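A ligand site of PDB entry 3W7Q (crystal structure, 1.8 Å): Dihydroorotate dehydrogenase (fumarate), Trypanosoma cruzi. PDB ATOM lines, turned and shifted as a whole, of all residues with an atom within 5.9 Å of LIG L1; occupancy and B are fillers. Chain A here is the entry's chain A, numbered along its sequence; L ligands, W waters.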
ATOM      1  N   LYS A  44      22.791  20.320 -10.362  1.00  0.00           N
ATOM      2  CA  LYS A  44      22.231  21.093  -9.318  1.00  0.00           C
ATOM      3  C   LYS A  44      22.717  20.619  -7.947  1.00  0.00           C
ATOM      4  O   LYS A  44      22.701  19.465  -7.669  1.00  0.00           O
ATOM      5  CB  LYS A  44      20.721  20.999  -9.328  1.00  0.00           C
ATOM      6  CG  LYS A  44      20.006  21.591  -8.129  1.00  0.00           C
ATOM      7  CD  LYS A  44      20.131  23.063  -7.959  1.00  0.00           C
ATOM      8  CE  LYS A  44      19.650  23.530  -6.572  1.00  0.00           C
ATOM      9  NZ  LYS A  44      19.696  25.064  -6.509  1.00  0.00           N
ATOM     10  N   SER A  45      23.072  21.585  -7.089  1.00  0.00           N
ATOM     11  CA  SER A  45      23.536  21.303  -5.718  1.00  0.00           C
ATOM     12  C   SER A  45      22.489  20.416  -5.058  1.00  0.00           C
ATOM     13  O   SER A  45      21.325  20.742  -5.066  1.00  0.00           O
ATOM     14  CB  SER A  45      23.800  22.548  -4.884  1.00  0.00           C
ATOM     15  OG  SER A  45      24.970  23.175  -5.357  1.00  0.00           O
ATOM     16  N   ARG A  51      14.115  17.781  -2.262  1.00  0.00           N
ATOM     17  CA  ARG A  51      13.601  19.013  -1.703  1.00  0.00           C
ATOM     18  C   ARG A  51      12.754  19.752  -2.720  1.00  0.00           C
ATOM     19  O   ARG A  51      13.108  19.859  -3.887  1.00  0.00           O
ATOM     20  CB  ARG A  51      14.682  20.008  -1.240  1.00  0.00           C
ATOM     21  CG  ARG A  51      15.555  19.521  -0.106  1.00  0.00           C
ATOM     22  CD  ARG A  51      16.657  20.482   0.259  1.00  0.00           C
ATOM     23  NE  ARG A  51      16.197  21.850   0.525  1.00  0.00           N
ATOM     24  CZ  ARG A  51      15.769  22.297   1.696  1.00  0.00           C
ATOM     25  NH1 ARG A  51      15.732  21.497   2.791  1.00  0.00           N
ATOM     26  NH2 ARG A  51      15.396  23.541   1.797  1.00  0.00           N
ATOM     27  N   ASN A  54      11.975  26.659  -1.787  1.00  0.00           N
ATOM     28  CA  ASN A  54      11.185  27.773  -1.233  1.00  0.00           C
ATOM     29  C   ASN A  54       9.960  28.068  -2.048  1.00  0.00           C
ATOM     30  O   ASN A  54       9.865  27.675  -3.210  1.00  0.00           O
ATOM     31  CB  ASN A  54      12.093  29.013  -1.125  1.00  0.00           C
ATOM     32  CG  ASN A  54      13.079  28.924   0.038  1.00  0.00           C
ATOM     33  OD1 ASN A  54      12.892  28.143   0.991  1.00  0.00           O
ATOM     34  ND2 ASN A  54      14.057  29.804   0.047  1.00  0.00           N
ATOM     35  N   ASN A  68      17.635  35.506  -6.496  1.00  0.00           N
ATOM     36  CA  ASN A  68      17.008  34.230  -6.189  1.00  0.00           C
ATOM     37  C   ASN A  68      17.073  33.849  -4.729  1.00  0.00           C
ATOM     38  O   ASN A  68      18.036  34.148  -4.021  1.00  0.00           O
ATOM     39  CB  ASN A  68      17.559  33.088  -7.074  1.00  0.00           C
ATOM     40  CG  ASN A  68      18.793  32.438  -6.481  1.00  0.00           C
ATOM     41  OD1 ASN A  68      18.693  31.640  -5.553  1.00  0.00           O
ATOM     42  ND2 ASN A  68      19.965  32.817  -6.956  1.00  0.00           N
ATOM     43  N   SER A  69      16.051  33.111  -4.280  1.00  0.00           N
ATOM     44  CA  SER A  69      16.119  32.403  -2.985  1.00  0.00           C
ATOM     45  C   SER A  69      15.464  31.054  -3.220  1.00  0.00           C
ATOM     46  O   SER A  69      14.403  30.749  -2.689  1.00  0.00           O
ATOM     47  CB  SER A  69      15.382  33.131  -1.875  1.00  0.00           C
ATOM     48  OG  SER A  69      15.577  32.482  -0.635  1.00  0.00           O
ATOM     49  N   MET A  70      16.100  30.233  -4.051  1.00  0.00           N
ATOM     50  CA  MET A  70      15.507  28.987  -4.471  1.00  0.00           C
ATOM     51  C   MET A  70      15.267  28.030  -3.296  1.00  0.00           C
ATOM     52  O   MET A  70      14.269  27.394  -3.231  1.00  0.00           O
ATOM     53  CB  MET A  70      16.366  28.287  -5.501  1.00  0.00           C
ATOM     54  CG  MET A  70      16.737  29.124  -6.686  1.00  0.00           C
ATOM     55  SD  MET A  70      15.337  29.599  -7.666  1.00  0.00           S
ATOM     56  CE  MET A  70      14.879  28.029  -8.318  1.00  0.00           C
ATOM     57  N   GLY A  71      16.213  27.972  -2.388  1.00  0.00           N
ATOM     58  CA  GLY A  71      16.125  27.059  -1.282  1.00  0.00           C
ATOM     59  C   GLY A  71      16.467  25.599  -1.519  1.00  0.00           C
ATOM     60  O   GLY A  71      15.915  24.755  -0.923  1.00  0.00           O
ATOM     61  N   LEU A  72      17.417  25.381  -2.415  1.00  0.00           N
ATOM     62  CA  LEU A  72      17.911  24.078  -2.747  1.00  0.00           C
ATOM     63  C   LEU A  72      16.875  23.072  -3.252  1.00  0.00           C
ATOM     64  O   LEU A  72      16.871  21.945  -2.846  1.00  0.00           O
ATOM     65  CB  LEU A  72      18.694  23.482  -1.589  1.00  0.00           C
ATOM     66  CG  LEU A  72      20.177  23.651  -1.487  1.00  0.00           C
ATOM     67  CD1 LEU A  72      20.675  23.157  -0.160  1.00  0.00           C
ATOM     68  CD2 LEU A  72      21.005  23.208  -2.680  1.00  0.00           C
ATOM     69  N   PRO A  73      16.001  23.496  -4.129  1.00  0.00           N
ATOM     70  CA  PRO A  73      15.115  22.454  -4.688  1.00  0.00           C
ATOM     71  C   PRO A  73      15.961  21.495  -5.495  1.00  0.00           C
ATOM     72  O   PRO A  73      16.728  21.933  -6.257  1.00  0.00           O
ATOM     73  CB  PRO A  73      14.169  23.218  -5.572  1.00  0.00           C
ATOM     74  CG  PRO A  73      14.928  24.341  -6.081  1.00  0.00           C
ATOM     75  CD  PRO A  73      15.759  24.794  -4.948  1.00  0.00           C
ATOM     76  N   SER A 100      25.528  20.099  -1.706  1.00  0.00           N
ATOM     77  CA  SER A 100      25.336  21.157  -0.773  1.00  0.00           C
ATOM     78  C   SER A 100      24.526  20.760   0.454  1.00  0.00           C
ATOM     79  O   SER A 100      23.474  21.253   0.670  1.00  0.00           O
ATOM     80  CB  SER A 100      24.751  22.365  -1.496  1.00  0.00           C
ATOM     81  OG  SER A 100      24.468  23.432  -0.686  1.00  0.00           O
ATOM     82  N   LEU A 102      23.188  20.396   4.279  1.00  0.00           N
ATOM     83  CA  LEU A 102      22.857  21.438   5.231  1.00  0.00           C
ATOM     84  C   LEU A 102      23.594  21.327   6.604  1.00  0.00           C
ATOM     85  O   LEU A 102      23.362  22.059   7.522  1.00  0.00           O
ATOM     86  CB  LEU A 102      21.334  21.538   5.386  1.00  0.00           C
ATOM     87  CG  LEU A 102      20.629  21.990   4.081  1.00  0.00           C
ATOM     88  CD1 LEU A 102      19.157  21.740   4.169  1.00  0.00           C
ATOM     89  CD2 LEU A 102      20.871  23.421   3.783  1.00  0.00           C
ATOM     90  N   ASN A 128      29.679  22.832  -2.351  1.00  0.00           N
ATOM     91  CA  ASN A 128      29.242  24.196  -2.185  1.00  0.00           C
ATOM     92  C   ASN A 128      29.367  24.636  -0.747  1.00  0.00           C
ATOM     93  O   ASN A 128      28.650  24.145   0.180  1.00  0.00           O
ATOM     94  CB  ASN A 128      27.733  24.284  -2.576  1.00  0.00           C
ATOM     95  CG  ASN A 128      27.196  25.689  -2.483  1.00  0.00           C
ATOM     96  OD1 ASN A 128      27.916  26.641  -2.471  1.00  0.00           O
ATOM     97  ND2 ASN A 128      25.934  25.815  -2.508  1.00  0.00           N
ATOM     98  N   SER A 130      29.051  27.965  -0.027  1.00  0.00           N
ATOM     99  CA  SER A 130      28.348  29.220   0.001  1.00  0.00           C
ATOM    100  C   SER A 130      26.970  28.783   0.301  1.00  0.00           C
ATOM    101  O   SER A 130      26.124  28.828  -0.579  1.00  0.00           O
ATOM    102  CB  SER A 130      28.407  29.940  -1.344  1.00  0.00           C
ATOM    103  OG  SER A 130      29.476  29.425  -2.177  1.00  0.00           O
ATOM    104  N   CYS A 131      26.737  28.312   1.528  1.00  0.00           N
ATOM    105  CA  CYS A 131      25.433  27.819   1.917  1.00  0.00           C
ATOM    106  C   CYS A 131      25.182  27.951   3.449  1.00  0.00           C
ATOM    107  O   CYS A 131      26.132  28.139   4.210  1.00  0.00           O
ATOM    108  CB  CYS A 131      25.339  26.354   1.504  1.00  0.00           C
ATOM    109  SG  CYS A 131      26.446  25.251   2.388  1.00  0.00           S
ATOM    110  N   PRO A 132      23.917  27.804   3.884  1.00  0.00           N
ATOM    111  CA  PRO A 132      23.548  27.721   5.310  1.00  0.00           C
ATOM    112  C   PRO A 132      24.049  26.544   6.107  1.00  0.00           C
ATOM    113  O   PRO A 132      24.106  25.405   5.661  1.00  0.00           O
ATOM    114  CB  PRO A 132      21.974  27.696   5.337  1.00  0.00           C
ATOM    115  CG  PRO A 132      21.532  28.081   3.962  1.00  0.00           C
ATOM    116  CD  PRO A 132      22.717  27.915   3.015  1.00  0.00           C
ATOM    117  N   LYS A 165      32.936  25.583  -4.160  1.00  0.00           N
ATOM    118  CA  LYS A 165      32.245  26.800  -4.642  1.00  0.00           C
ATOM    119  C   LYS A 165      32.177  27.779  -3.479  1.00  0.00           C
ATOM    120  O   LYS A 165      31.690  27.462  -2.399  1.00  0.00           O
ATOM    121  CB  LYS A 165      30.823  26.412  -5.080  1.00  0.00           C
ATOM    122  CG  LYS A 165      29.975  27.536  -5.576  1.00  0.00           C
ATOM    123  CD  LYS A 165      30.357  28.031  -6.980  1.00  0.00           C
ATOM    124  CE  LYS A 165      29.263  28.908  -7.571  1.00  0.00           C
ATOM    125  NZ  LYS A 165      28.031  28.226  -8.003  1.00  0.00           N
ATOM    126  N   ASN A 195      29.853  32.325  -6.022  1.00  0.00           N
ATOM    127  CA  ASN A 195      28.427  32.172  -5.814  1.00  0.00           C
ATOM    128  C   ASN A 195      27.789  33.590  -5.771  1.00  0.00           C
ATOM    129  O   ASN A 195      28.452  34.548  -5.994  1.00  0.00           O
ATOM    130  CB  ASN A 195      28.140  31.348  -4.552  1.00  0.00           C
ATOM    131  CG  ASN A 195      26.896  30.477  -4.668  1.00  0.00           C
ATOM    132  OD1 ASN A 195      25.870  30.927  -5.003  1.00  0.00           O
ATOM    133  ND2 ASN A 195      27.032  29.209  -4.384  1.00  0.00           N
ATOM    134  N   SER A 196      26.484  33.672  -5.597  1.00  0.00           N
ATOM    135  CA  SER A 196      25.788  34.926  -5.672  1.00  0.00           C
ATOM    136  C   SER A 196      26.298  35.916  -4.646  1.00  0.00           C
ATOM    137  O   SER A 196      26.820  35.531  -3.646  1.00  0.00           O
ATOM    138  CB  SER A 196      24.299  34.798  -5.355  1.00  0.00           C
ATOM    139  OG  SER A 196      23.845  33.537  -5.336  1.00  0.00           O
ATOM    140  N   LYS A 215      11.967  35.063   2.403  1.00  0.00           N
ATOM    141  CA  LYS A 215      12.931  35.901   3.117  1.00  0.00           C
ATOM    142  C   LYS A 215      12.670  37.400   2.893  1.00  0.00           C
ATOM    143  O   LYS A 215      13.606  38.180   2.813  1.00  0.00           O
ATOM    144  CB  LYS A 215      14.349  35.554   2.674  1.00  0.00           C
ATOM    145  CG  LYS A 215      14.738  34.126   2.981  1.00  0.00           C
ATOM    146  CD  LYS A 215      15.677  33.583   1.947  1.00  0.00           C
ATOM    147  CE  LYS A 215      16.868  34.492   1.648  1.00  0.00           C
ATOM    148  NZ  LYS A 215      17.246  34.452   0.252  1.00  0.00           N
ATOM    149  N   GLY A 220      20.104  36.060  -3.325  1.00  0.00           N
ATOM    150  CA  GLY A 220      21.392  36.280  -3.920  1.00  0.00           C
ATOM    151  C   GLY A 220      21.309  36.868  -5.332  1.00  0.00           C
ATOM    152  O   GLY A 220      20.418  36.550  -6.127  1.00  0.00           O
HETATM  153  O1  LIG L   1      18.837  28.969  -3.391  1.00  0.00           O
HETATM  154  C1  LIG L   1      19.632  28.091  -3.782  1.00  0.00           C
HETATM  155  O2  LIG L   1      19.284  26.889  -3.979  1.00  0.00           O
HETATM  156  C2  LIG L   1      20.968  28.535  -4.054  1.00  0.00           C
HETATM  157  N1  LIG L   1      20.974  29.748  -4.777  1.00  0.00           N
HETATM  158  C3  LIG L   1      22.195  30.351  -5.130  1.00  0.00           C
HETATM  159  O3  LIG L   1      22.180  31.424  -5.695  1.00  0.00           O
HETATM  160  N2  LIG L   1      23.346  29.762  -4.711  1.00  0.00           N
HETATM  161  C4  LIG L   1      23.378  28.601  -3.938  1.00  0.00           C
HETATM  162  O4  LIG L   1      24.478  28.158  -3.548  1.00  0.00           O
HETATM  163  C5  LIG L   1      22.128  27.952  -3.613  1.00  0.00           C
HETATM  164  C6  LIG L   1      22.115  26.802  -2.821  1.00  0.00           C
HETATM  165  C7  LIG L   1      22.473  27.094  -1.316  1.00  0.00           C
HETATM  166  C8  LIG L   1      21.365  27.522  -0.546  1.00  0.00           C
HETATM  167  C9  LIG L   1      20.882  28.838  -0.716  1.00  0.00           C
HETATM  168  C10 LIG L   1      20.654  26.675   0.316  1.00  0.00           C
HETATM  169  C11 LIG L   1      19.561  27.194   1.025  1.00  0.00           C
HETATM  170  C12 LIG L   1      19.106  28.453   0.801  1.00  0.00           C
HETATM  171  C13 LIG L   1      19.780  29.266  -0.071  1.00  0.00           C
HETATM  172  C14 LIG L   1      19.150  30.548  -0.182  1.00  0.00           C
HETATM  173  C15 LIG L   1      17.834  30.425   0.559  1.00  0.00           C
HETATM  174  N3  LIG L   1      18.007  29.142   1.272  1.00  0.00           N
HETATM  175  C16 LIG L   1      17.078  28.777   2.172  1.00  0.00           C
HETATM  176  O5  LIG L   1      16.116  29.520   2.471  1.00  0.00           O
HETATM  177  O6  LIG L   1      17.387  27.660   2.844  1.00  0.00           O
HETATM  178  C17 LIG L   1      16.532  26.990   3.809  1.00  0.00           C
HETATM  179  C18 LIG L   1      17.259  25.682   4.122  1.00  0.00           C
HETATM  180  C19 LIG L   1      16.516  27.874   5.009  1.00  0.00           C
HETATM  181  C20 LIG L   1      15.108  26.724   3.215  1.00  0.00           C
HETATM  182  N1  LG2 L   2      25.135  27.900  -6.908  1.00  0.00           N
HETATM  183  C1  LG2 L   2      25.456  26.708  -6.368  1.00  0.00           C
HETATM  184  O1  LG2 L   2      26.665  26.508  -6.084  1.00  0.00           O
HETATM  185  N2  LG2 L   2      24.523  25.750  -6.198  1.00  0.00           N
HETATM  186  C2  LG2 L   2      23.225  25.915  -6.532  1.00  0.00           C
HETATM  187  O2  LG2 L   2      22.330  24.998  -6.472  1.00  0.00           O
HETATM  188  C3  LG2 L   2      22.850  27.156  -7.125  1.00  0.00           C
HETATM  189  N3  LG2 L   2      21.626  27.379  -7.576  1.00  0.00           N
HETATM  190  C4  LG2 L   2      21.327  28.565  -8.237  1.00  0.00           C
HETATM  191  C5  LG2 L   2      20.075  28.749  -8.815  1.00  0.00           C
HETATM  192  C6  LG2 L   2      19.739  29.884  -9.504  1.00  0.00           C
HETATM  193  C7  LG2 L   2      18.354  30.106 -10.123  1.00  0.00           C
HETATM  194  C8  LG2 L   2      20.746  30.887  -9.750  1.00  0.00           C
HETATM  195  C9  LG2 L   2      20.373  32.112 -10.517  1.00  0.00           C
HETATM  196  C10 LG2 L   2      22.009  30.718  -9.227  1.00  0.00           C
HETATM  197  C11 LG2 L   2      22.347  29.584  -8.492  1.00  0.00           C
HETATM  198  N4  LG2 L   2      23.595  29.352  -7.975  1.00  0.00           N
HETATM  199  C12 LG2 L   2      23.878  28.165  -7.354  1.00  0.00           C
HETATM  200  C13 LG2 L   2      24.654  30.341  -8.156  1.00  0.00           C
HETATM  201  C14 LG2 L   2      25.237  30.285  -9.505  1.00  0.00           C
HETATM  202  O3  LG2 L   2      25.870  29.016  -9.614  1.00  0.00           O
HETATM  203  C15 LG2 L   2      26.228  31.429  -9.683  1.00  0.00           C
HETATM  204  O4  LG2 L   2      27.269  31.202  -8.746  1.00  0.00           O
HETATM  205  C16 LG2 L   2      25.678  32.859  -9.487  1.00  0.00           C
HETATM  206  O5  LG2 L   2      24.386  32.910 -10.122  1.00  0.00           O
HETATM  207  C17 LG2 L   2      26.606  33.862 -10.209  1.00  0.00           C
HETATM  208  O6  LG2 L   2      26.771  33.687 -11.616  1.00  0.00           O
HETATM  209  P1  LG2 L   2      26.002  34.531 -12.710  1.00  0.00           P
HETATM  210  O7  LG2 L   2      26.462  33.934 -14.025  1.00  0.00           O
HETATM  211  O8  LG2 L   2      26.348  35.970 -12.449  1.00  0.00           O
HETATM  212  O9  LG2 L   2      24.532  34.283 -12.354  1.00  0.00           O
HETATM  213  O   HOH W   1      19.304  33.848  -0.852  1.00  0.00           O
HETATM  214  O   HOH W   2      22.797  32.359  -3.171  1.00  0.00           O
HETATM  215  O   HOH W   3      20.230  32.478  -3.078  1.00  0.00           O
HETATM  216  O   HOH W   4      12.562  25.205   1.517  1.00  0.00           O
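ND2 of Asn 68 is in hydrogen-bond range of O3 of LIG L1 (2.9 Å). The side-chain amino group (NZ) of Lys 165 lies within hydrogen-bond range of an oxygen (O3) of LG2 L2. N of Met 70 is in hydrogen-bond range of O1 of LIG L1, at 3.1 Å. A nitrogen (N2) of LG2 L2 sits at hydrogen-bond distance from the side-chain hydroxyl of Ser 45, 2.7 Å away. O3 of LIG L1 is in hydrogen-bond range of OG of Ser 196 (2.7 Å). ND2 of Asn 54 sits at hydrogen-bond distance from O5 of LIG L1, 3.2 Å away. O4 of LIG L1 sits at hydrogen-bond distance from ND2 of Asn 128. O1 of LIG L1 is in hydrogen-bond range of N of Gly 71 (3.0 Å). The backbone NH of Leu 72 sits at hydrogen-bond distance from an oxygen (O2) of LIG L1 (2.9 Å). The side-chain amino group (NZ) of Lys 44 is in salt-bridge range of an oxygen (O2) of LIG L1 (3.1 Å). N2 of LIG L1 is in hydrogen-bond range of OD1 of Asn 195. An oxygen (O1) of LG2 L2 lies within hydrogen-bond range of the side-chain amide nitrogen (ND2) of Asn 195, 3.2 Å away. O2 of LG2 L2 lies within hydrogen-bond range of NZ of Lys 44 (2.6 Å).
Water W2 bridges the side-chain hydroxyl (OG) of Ser 196 (2.7 Å) and an oxygen (O3) of LIG L1 (2.8 Å). Water W3 bridges the backbone carbonyl oxygen of Asn 68 (2.9 Å) and a nitrogen (N1) of LIG L1 (3.3 Å). Water W1 lies within hydrogen-bond range of NZ of Lys 215 (2.4 Å), N of Gly 220 (3.4 Å) and O of Asn 68 (3.4 Å). Water W4 bridges OD1 of Asn 54 (3.0 Å) and NH2 of Arg 51 (3.3 Å).
The backbone carbonyl oxygen of Ser 130 lies close to an oxygen (O4) of LIG L1. Arg 51 touches LIG L1. Ser 69 touches LIG L1. CD of Pro 132 touches C10 of LIG L1, 3.6 Å away. Hydrophobic or aromatic side chains that line LIG L1: Met 70, Leu 72 and Pro 132. Along chain A the residues within 4 Å of LIG L1 span positions 44 to 196.
A nitrogen (N1) of LG2 L2 sits close to a nitrogen (N2) of LIG L1, at 3.4 Å.
ND2 of Asn 195 sits at hydrogen-bond distance from OD1 of Asn 128, at 3.3 Å. The guanidinium group (NH2) of Arg 51 lies within hydrogen-bond range of the backbone carbonyl oxygen (O) of Gly 71 (3.0 Å). O of Lys 165 lies within hydrogen-bond range of OG of Ser 130, 3.0 Å away. O of Asn 128 lies within hydrogen-bond range of SG of Cys 131 (3.3 Å). OD1 of Asn 68 lies within hydrogen-bond range of N of Met 70 (3.3 Å). NZ of Lys 215 is in hydrogen-bond range of OG of Ser 69. The side-chain amide oxygen (OD1) of Asn 128 lies within hydrogen-bond range of the backbone NH (N) of Ser 130 (3.0 Å). O of Met 70 sits at hydrogen-bond distance from N of Asn 54.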
